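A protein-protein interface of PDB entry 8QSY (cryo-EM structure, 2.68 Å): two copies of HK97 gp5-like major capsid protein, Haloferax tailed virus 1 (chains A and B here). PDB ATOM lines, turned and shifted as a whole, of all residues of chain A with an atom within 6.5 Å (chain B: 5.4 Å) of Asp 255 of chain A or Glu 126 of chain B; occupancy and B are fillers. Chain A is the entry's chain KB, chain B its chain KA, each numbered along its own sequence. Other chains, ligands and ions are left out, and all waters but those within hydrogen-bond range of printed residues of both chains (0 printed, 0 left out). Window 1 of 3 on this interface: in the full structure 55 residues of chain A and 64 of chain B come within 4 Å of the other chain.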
ATOM      1  N   ASP A 152      19.175 -18.089  20.858  1.00  0.00           N
ATOM      2  CA  ASP A 152      19.056 -16.934  21.739  1.00  0.00           C
ATOM      3  C   ASP A 152      18.310 -15.783  21.060  1.00  0.00           C
ATOM      4  O   ASP A 152      18.354 -15.636  19.837  1.00  0.00           O
ATOM      5  CB  ASP A 152      20.436 -16.392  22.101  1.00  0.00           C
ATOM      6  CG  ASP A 152      21.331 -17.363  22.852  1.00  0.00           C
ATOM      7  OD1 ASP A 152      20.811 -18.368  23.386  1.00  0.00           O
ATOM      8  OD2 ASP A 152      22.556 -17.107  22.915  1.00  0.00           O
ATOM      9  N   GLU A 153      17.645 -14.941  21.870  1.00  0.00           N
ATOM     10  CA  GLU A 153      17.010 -13.739  21.341  1.00  0.00           C
ATOM     11  C   GLU A 153      18.039 -12.635  21.060  1.00  0.00           C
ATOM     12  O   GLU A 153      19.117 -12.607  21.652  1.00  0.00           O
ATOM     13  CB  GLU A 153      15.855 -13.289  22.234  1.00  0.00           C
ATOM     14  CG  GLU A 153      16.284 -12.669  23.550  1.00  0.00           C
ATOM     15  CD  GLU A 153      15.129 -12.058  24.330  1.00  0.00           C
ATOM     16  OE1 GLU A 153      14.328 -11.322  23.723  1.00  0.00           O
ATOM     17  OE2 GLU A 153      15.026 -12.314  25.541  1.00  0.00           O
ATOM     18  N   GLU A 250      27.447 -15.980  37.787  1.00  0.00           N
ATOM     19  CA  GLU A 250      27.986 -16.470  36.526  1.00  0.00           C
ATOM     20  C   GLU A 250      26.878 -16.938  35.580  1.00  0.00           C
ATOM     21  O   GLU A 250      26.916 -16.608  34.398  1.00  0.00           O
ATOM     22  CB  GLU A 250      29.015 -17.569  36.776  1.00  0.00           C
ATOM     23  CG  GLU A 250      30.311 -17.051  37.369  1.00  0.00           C
ATOM     24  CD  GLU A 250      31.010 -16.032  36.484  1.00  0.00           C
ATOM     25  OE1 GLU A 250      31.359 -16.381  35.334  1.00  0.00           O
ATOM     26  OE2 GLU A 250      31.172 -14.873  36.931  1.00  0.00           O
ATOM     27  N   VAL A 251      25.875 -17.663  36.089  1.00  0.00           N
ATOM     28  CA  VAL A 251      24.744 -18.089  35.274  1.00  0.00           C
ATOM     29  C   VAL A 251      23.907 -16.880  34.847  1.00  0.00           C
ATOM     30  O   VAL A 251      23.517 -16.784  33.687  1.00  0.00           O
ATOM     31  CB  VAL A 251      23.906 -19.165  35.990  1.00  0.00           C
ATOM     32  CG1 VAL A 251      22.734 -19.613  35.144  1.00  0.00           C
ATOM     33  CG2 VAL A 251      24.743 -20.381  36.323  1.00  0.00           C
ATOM     34  N   ASP A 252      23.675 -15.931  35.760  1.00  0.00           N
ATOM     35  CA  ASP A 252      22.907 -14.715  35.522  1.00  0.00           C
ATOM     36  C   ASP A 252      23.558 -13.808  34.464  1.00  0.00           C
ATOM     37  O   ASP A 252      22.853 -13.141  33.705  1.00  0.00           O
ATOM     38  CB  ASP A 252      22.714 -13.997  36.856  1.00  0.00           C
ATOM     39  CG  ASP A 252      21.742 -12.831  36.847  1.00  0.00           C
ATOM     40  OD1 ASP A 252      20.778 -12.855  36.047  1.00  0.00           O
ATOM     41  OD2 ASP A 252      21.933 -11.913  37.677  1.00  0.00           O
ATOM     42  N   LYS A 253      24.890 -13.826  34.348  1.00  0.00           N
ATOM     43  CA  LYS A 253      25.613 -13.113  33.301  1.00  0.00           C
ATOM     44  C   LYS A 253      25.398 -13.689  31.902  1.00  0.00           C
ATOM     45  O   LYS A 253      25.620 -12.980  30.924  1.00  0.00           O
ATOM     46  CB  LYS A 253      27.092 -13.040  33.653  1.00  0.00           C
ATOM     47  CG  LYS A 253      27.354 -12.041  34.757  1.00  0.00           C
ATOM     48  CD  LYS A 253      28.560 -12.359  35.619  1.00  0.00           C
ATOM     49  CE  LYS A 253      29.902 -12.137  34.955  1.00  0.00           C
ATOM     50  NZ  LYS A 253      30.998 -12.183  35.950  1.00  0.00           N
ATOM     51  N   ASP A 254      24.944 -14.944  31.790  1.00  0.00           N
ATOM     52  CA  ASP A 254      24.478 -15.500  30.525  1.00  0.00           C
ATOM     53  C   ASP A 254      22.949 -15.435  30.402  1.00  0.00           C
ATOM     54  O   ASP A 254      22.378 -16.014  29.484  1.00  0.00           O
ATOM     55  CB  ASP A 254      24.990 -16.930  30.325  1.00  0.00           C
ATOM     56  CG  ASP A 254      26.506 -17.115  30.277  1.00  0.00           C
ATOM     57  OD1 ASP A 254      27.288 -16.152  30.338  1.00  0.00           O
ATOM     58  OD2 ASP A 254      26.944 -18.264  30.202  1.00  0.00           O
ATOM     59  N   ASP A 255      22.265 -14.743  31.323  1.00  0.00           N
ATOM     60  CA  ASP A 255      20.819 -14.505  31.308  1.00  0.00           C
ATOM     61  C   ASP A 255      19.968 -15.775  31.433  1.00  0.00           C
ATOM     62  O   ASP A 255      18.854 -15.828  30.909  1.00  0.00           O
ATOM     63  CB  ASP A 255      20.415 -13.574  30.161  1.00  0.00           C
ATOM     64  CG  ASP A 255      21.172 -12.259  30.191  1.00  0.00           C
ATOM     65  OD1 ASP A 255      21.003 -11.499  31.168  1.00  0.00           O
ATOM     66  OD2 ASP A 255      21.918 -12.002  29.230  1.00  0.00           O
ATOM     67  N   PHE A 256      20.469 -16.778  32.165  1.00  0.00           N
ATOM     68  CA  PHE A 256      19.638 -17.859  32.687  1.00  0.00           C
ATOM     69  C   PHE A 256      19.446 -17.700  34.200  1.00  0.00           C
ATOM     70  O   PHE A 256      20.249 -17.042  34.857  1.00  0.00           O
ATOM     71  CB  PHE A 256      20.267 -19.215  32.356  1.00  0.00           C
ATOM     72  CG  PHE A 256      20.319 -19.520  30.878  1.00  0.00           C
ATOM     73  CD1 PHE A 256      19.206 -20.038  30.227  1.00  0.00           C
ATOM     74  CD2 PHE A 256      21.457 -19.254  30.126  1.00  0.00           C
ATOM     75  CE1 PHE A 256      19.226 -20.288  28.860  1.00  0.00           C
ATOM     76  CE2 PHE A 256      21.468 -19.493  28.757  1.00  0.00           C
ATOM     77  CZ  PHE A 256      20.362 -20.016  28.125  1.00  0.00           C
ATOM     78  N   ARG A 257      18.409 -18.342  34.766  1.00  0.00           N
ATOM     79  CA  ARG A 257      18.156 -18.310  36.203  1.00  0.00           C
ATOM     80  C   ARG A 257      18.296 -19.722  36.770  1.00  0.00           C
ATOM     81  O   ARG A 257      17.450 -20.565  36.494  1.00  0.00           O
ATOM     82  CB  ARG A 257      16.770 -17.711  36.486  1.00  0.00           C
ATOM     83  CG  ARG A 257      16.559 -17.291  37.934  1.00  0.00           C
ATOM     84  CD  ARG A 257      17.128 -15.935  38.339  1.00  0.00           C
ATOM     85  NE  ARG A 257      16.136 -14.859  38.406  1.00  0.00           N
ATOM     86  CZ  ARG A 257      15.376 -14.572  39.464  1.00  0.00           C
ATOM     87  NH1 ARG A 257      14.509 -13.575  39.401  1.00  0.00           N
ATOM     88  NH2 ARG A 257      15.480 -15.275  40.579  1.00  0.00           N
ATOM     89  N   GLY B 124      16.037 -20.378  24.076  1.00  0.00           N
ATOM     90  CA  GLY B 124      17.375 -19.810  24.171  1.00  0.00           C
ATOM     91  C   GLY B 124      17.511 -18.842  25.349  1.00  0.00           C
ATOM     92  O   GLY B 124      16.625 -18.739  26.196  1.00  0.00           O
ATOM     93  N   ARG B 125      18.638 -18.119  25.384  1.00  0.00           N
ATOM     94  CA  ARG B 125      18.869 -17.020  26.311  1.00  0.00           C
ATOM     95  C   ARG B 125      17.754 -15.975  26.187  1.00  0.00           C
ATOM     96  O   ARG B 125      17.418 -15.563  25.079  1.00  0.00           O
ATOM     97  CB  ARG B 125      20.248 -16.447  25.978  1.00  0.00           C
ATOM     98  CG  ARG B 125      20.652 -15.176  26.705  1.00  0.00           C
ATOM     99  CD  ARG B 125      21.966 -14.661  26.141  1.00  0.00           C
ATOM    100  NE  ARG B 125      22.560 -13.615  26.960  1.00  0.00           N
ATOM    101  CZ  ARG B 125      23.836 -13.243  26.918  1.00  0.00           C
ATOM    102  NH1 ARG B 125      24.261 -12.285  27.721  1.00  0.00           N
ATOM    103  NH2 ARG B 125      24.685 -13.829  26.089  1.00  0.00           N
ATOM    104  N   GLU B 126      17.181 -15.568  27.332  1.00  0.00           N
ATOM    105  CA  GLU B 126      16.129 -14.553  27.408  1.00  0.00           C
ATOM    106  C   GLU B 126      16.611 -13.352  28.231  1.00  0.00           C
ATOM    107  O   GLU B 126      16.908 -13.496  29.416  1.00  0.00           O
ATOM    108  CB  GLU B 126      14.835 -15.170  27.963  1.00  0.00           C
ATOM    109  CG  GLU B 126      13.716 -14.183  28.310  1.00  0.00           C
ATOM    110  CD  GLU B 126      12.754 -13.761  27.205  1.00  0.00           C
ATOM    111  OE1 GLU B 126      12.527 -14.556  26.264  1.00  0.00           O
ATOM    112  OE2 GLU B 126      12.199 -12.642  27.300  1.00  0.00           O
ATOM    113  N   LEU B 127      16.662 -12.160  27.613  1.00  0.00           N
ATOM    114  CA  LEU B 127      17.142 -10.947  28.266  1.00  0.00           C
ATOM    115  C   LEU B 127      16.038 -10.292  29.092  1.00  0.00           C
ATOM    116  O   LEU B 127      14.873 -10.271  28.695  1.00  0.00           O
ATOM    117  CB  LEU B 127      17.657  -9.965  27.211  1.00  0.00           C
ATOM    118  CG  LEU B 127      18.704 -10.521  26.253  1.00  0.00           C
ATOM    119  CD1 LEU B 127      19.195  -9.420  25.341  1.00  0.00           C
ATOM    120  CD2 LEU B 127      19.872 -11.132  27.005  1.00  0.00           C
ATOM    121  N   ARG B 128      16.432  -9.690  30.221  1.00  0.00           N
ATOM    122  CA  ARG B 128      15.522  -8.988  31.120  1.00  0.00           C
ATOM    123  C   ARG B 128      14.990  -7.715  30.465  1.00  0.00           C
ATOM    124  O   ARG B 128      15.747  -6.958  29.861  1.00  0.00           O
ATOM    125  CB  ARG B 128      16.241  -8.673  32.435  1.00  0.00           C
ATOM    126  CG  ARG B 128      16.618  -9.920  33.211  1.00  0.00           C
ATOM    127  CD  ARG B 128      17.511  -9.546  34.365  1.00  0.00           C
ATOM    128  NE  ARG B 128      18.059 -10.644  35.127  1.00  0.00           N
ATOM    129  CZ  ARG B 128      17.651 -11.043  36.328  1.00  0.00           C
ATOM    130  NH1 ARG B 128      18.292 -12.021  36.940  1.00  0.00           N
ATOM    131  NH2 ARG B 128      16.613 -10.490  36.931  1.00  0.00           N
ATOM    132  N   LYS B 129      13.675  -7.490  30.604  1.00  0.00           N
ATOM    133  CA  LYS B 129      12.965  -6.374  29.993  1.00  0.00           C
ATOM    134  C   LYS B 129      12.288  -5.559  31.095  1.00  0.00           C
ATOM    135  O   LYS B 129      11.456  -6.096  31.823  1.00  0.00           O
ATOM    136  CB  LYS B 129      11.967  -6.921  28.964  1.00  0.00           C
ATOM    137  CG  LYS B 129      12.618  -7.613  27.774  1.00  0.00           C
ATOM    138  CD  LYS B 129      11.696  -8.547  27.025  1.00  0.00           C
ATOM    139  CE  LYS B 129      12.379  -9.255  25.874  1.00  0.00           C
ATOM    140  NZ  LYS B 129      13.288 -10.332  26.326  1.00  0.00           N
ATOM    141  N   GLN B 206       6.686 -13.974  18.546  1.00  0.00           N
ATOM    142  CA  GLN B 206       7.249 -13.846  19.880  1.00  0.00           C
ATOM    143  C   GLN B 206       8.709 -13.372  19.818  1.00  0.00           C
ATOM    144  O   GLN B 206       9.081 -12.464  20.553  1.00  0.00           O
ATOM    145  CB  GLN B 206       7.015 -15.140  20.661  1.00  0.00           C
ATOM    146  CG  GLN B 206       7.164 -14.997  22.176  1.00  0.00           C
ATOM    147  CD  GLN B 206       8.576 -15.018  22.731  1.00  0.00           C
ATOM    148  OE1 GLN B 206       9.548 -15.323  22.039  1.00  0.00           O
ATOM    149  NE2 GLN B 206       8.701 -14.718  24.018  1.00  0.00           N
ATOM    150  N   ALA B 210       9.917  -9.720  21.250  1.00  0.00           N
ATOM    151  CA  ALA B 210      10.978  -9.700  22.247  1.00  0.00           C
ATOM    152  C   ALA B 210      12.199  -8.911  21.759  1.00  0.00           C
ATOM    153  O   ALA B 210      12.826  -8.187  22.532  1.00  0.00           O
ATOM    154  CB  ALA B 210      11.313 -11.115  22.634  1.00  0.00           C
ATOM    155  N   PRO B 265      24.442  -7.415  36.467  1.00  0.00           N
ATOM    156  CA  PRO B 265      24.679  -8.669  37.192  1.00  0.00           C
ATOM    157  C   PRO B 265      25.878  -8.713  38.137  1.00  0.00           C
ATOM    158  O   PRO B 265      25.774  -9.300  39.211  1.00  0.00           O
ATOM    159  CB  PRO B 265      24.921  -9.686  36.066  1.00  0.00           C
ATOM    160  CG  PRO B 265      24.062  -9.182  34.938  1.00  0.00           C
ATOM    161  CD  PRO B 265      24.167  -7.677  35.052  1.00  0.00           C
ATOM    162  N   SER B 311      20.012  -7.008  32.147  1.00  0.00           N
ATOM    163  CA  SER B 311      20.947  -7.972  31.580  1.00  0.00           C
ATOM    164  C   SER B 311      22.246  -7.302  31.140  1.00  0.00           C
ATOM    165  O   SER B 311      22.245  -6.150  30.709  1.00  0.00           O
ATOM    166  CB  SER B 311      20.313  -8.668  30.413  1.00  0.00           C
ATOM    167  OG  SER B 311      19.320  -9.561  30.874  1.00  0.00           O
ATOM    168  N   SER B 312      23.344  -8.071  31.133  1.00  0.00           N
ATOM    169  CA  SER B 312      24.682  -7.607  30.771  1.00  0.00           C
ATOM    170  C   SER B 312      24.764  -7.098  29.321  1.00  0.00           C
ATOM    171  O   SER B 312      25.393  -6.077  29.045  1.00  0.00           O
ATOM    172  CB  SER B 312      25.685  -8.697  31.044  1.00  0.00           C
ATOM    173  OG  SER B 312      27.002  -8.226  30.828  1.00  0.00           O
ATOM    174  N   ALA B 313      24.099  -7.786  28.384  1.00  0.00           N
ATOM    175  CA  ALA B 313      24.148  -7.474  26.955  1.00  0.00           C
ATOM    176  C   ALA B 313      23.389  -6.200  26.549  1.00  0.00           C
ATOM    177  O   ALA B 313      23.480  -5.778  25.391  1.00  0.00           O
ATOM    178  CB  ALA B 313      23.632  -8.659  26.176  1.00  0.00           C
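Of chain B, only Arg 125, Glu 126, Leu 127 and Ser 311 come within 4 Å of Asp 255 of chain A. Of chain A, only Glu 153 (3.1 Å) and Asp 255 (3.4 Å) come within 4 Å of Glu 126 of chain B. Printed residues of chain B within 4 Å of Glu 153 of chain A: Arg 125, Glu 126, Leu 127, Lys 129 and Ala 210. Of the printed residues of chain A, Pro 265 of chain B touches Lys 253 (3.6 Å). Of the printed residues of chain B, Arg 257 of chain A touches Arg 128. Ser 312 of chain B touches none of the printed residues of chain A.
Among the printed residues, pairs that only touch across the chains: Asp 255 of chain A with Leu 127 of chain B (3.1 Å), Glu 153 of chain A with Ala 210 of chain B (3.2 Å), Lys 253 of chain A with Arg 125 of chain B (3.5 Å), Lys 253 of chain A with Pro 265 of chain B (3.6 Å), Phe 256 of chain A with Arg 125 of chain B (3.8 Å), Asp 152 of chain A with Gly 124 of chain B (3.8 Å) and Arg 257 of chain A with Arg 128 of chain B (3.9 Å).
No position is printed for both chains.
Printed residues of chain A that touch a printed residue of chain B: Asp 152, Glu 153, Asp 252, Lys 253, Asp 254, Asp 255, Phe 256 and Arg 257. Hydrophobic or aromatic side chains of chain A that line the printed part of chain B: Phe 256. Along chain A the printed residues that touch a printed residue of chain B span positions 152 to 257. Of the 12 printed residues of chain B, 9 touch a printed residue of chain A. Along chain B the printed residues that touch a printed residue of chain A span positions 124 to 311. Among the printed residues, 17 pairs touch across the chains.
OE2 of Glu 153 of chain A sits at hydrogen-bond distance from N of Leu 127 of chain B, 2.6 Å away. The backbone carbonyl oxygen (O) of Arg 125 of chain B lies within hydrogen-bond range of the backbone NH (N) of Glu 153 of chain A, at 3.3 Å. The side-chain carboxylate (OD2) of Asp 255 of chain A is in salt-bridge range of the guanidinium group (NH1) of Arg 125 of chain B (2.8 Å). The side-chain carboxylate (OD1) of Asp 252 of chain A lies within salt-bridge range of the guanidinium group (NH1) of Arg 128 of chain B. N of Arg 125 of chain B is in hydrogen-bond range of OD1 of Asp 152 of chain A (3.0 Å). The side-chain carboxylate of Glu 153 of chain A is in salt-bridge range of the side-chain amino group of Lys 129 of chain B. The side-chain carboxylate (OE2) of Glu 153 of chain A sits close to the side-chain carboxylate (OE2) of Glu 126 of chain B. The side-chain carboxylate (OD1) of Asp 255 of chain A is in hydrogen-bond range of the side-chain hydroxyl (OG) of Ser 311 of chain B (2.6 Å). The backbone carbonyl oxygen (O) of Asp 254 of chain A lies close to the guanidinium group (NE) of Arg 125 of chain B, at 3.5 Å. O of Asp 255 of chain A lies close to O of Glu 126 of chain B (3.4 Å).
The backbone carbonyl oxygen (O) of Leu 127 of chain B lies within hydrogen-bond range of the side-chain amino group (NZ) of Lys 129 of chain B (2.9 Å). NZ of Lys 253 of chain A lies within salt-bridge range of OE2 of Glu 250 of chain A, 2.9 Å away. The backbone NH (N) of Arg 128 of chain B sits at hydrogen-bond distance from the side-chain hydroxyl (OG) of Ser 311 of chain B. The side-chain carboxylate (OE2) of Glu 126 of chain B lies within salt-bridge range of the side-chain amino group (NZ) of Lys 129 of chain B. The backbone carbonyl oxygen (O) of Val 251 of chain A is in hydrogen-bond range of the backbone NH (N) of Phe 256 of chain A (3.4 Å).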
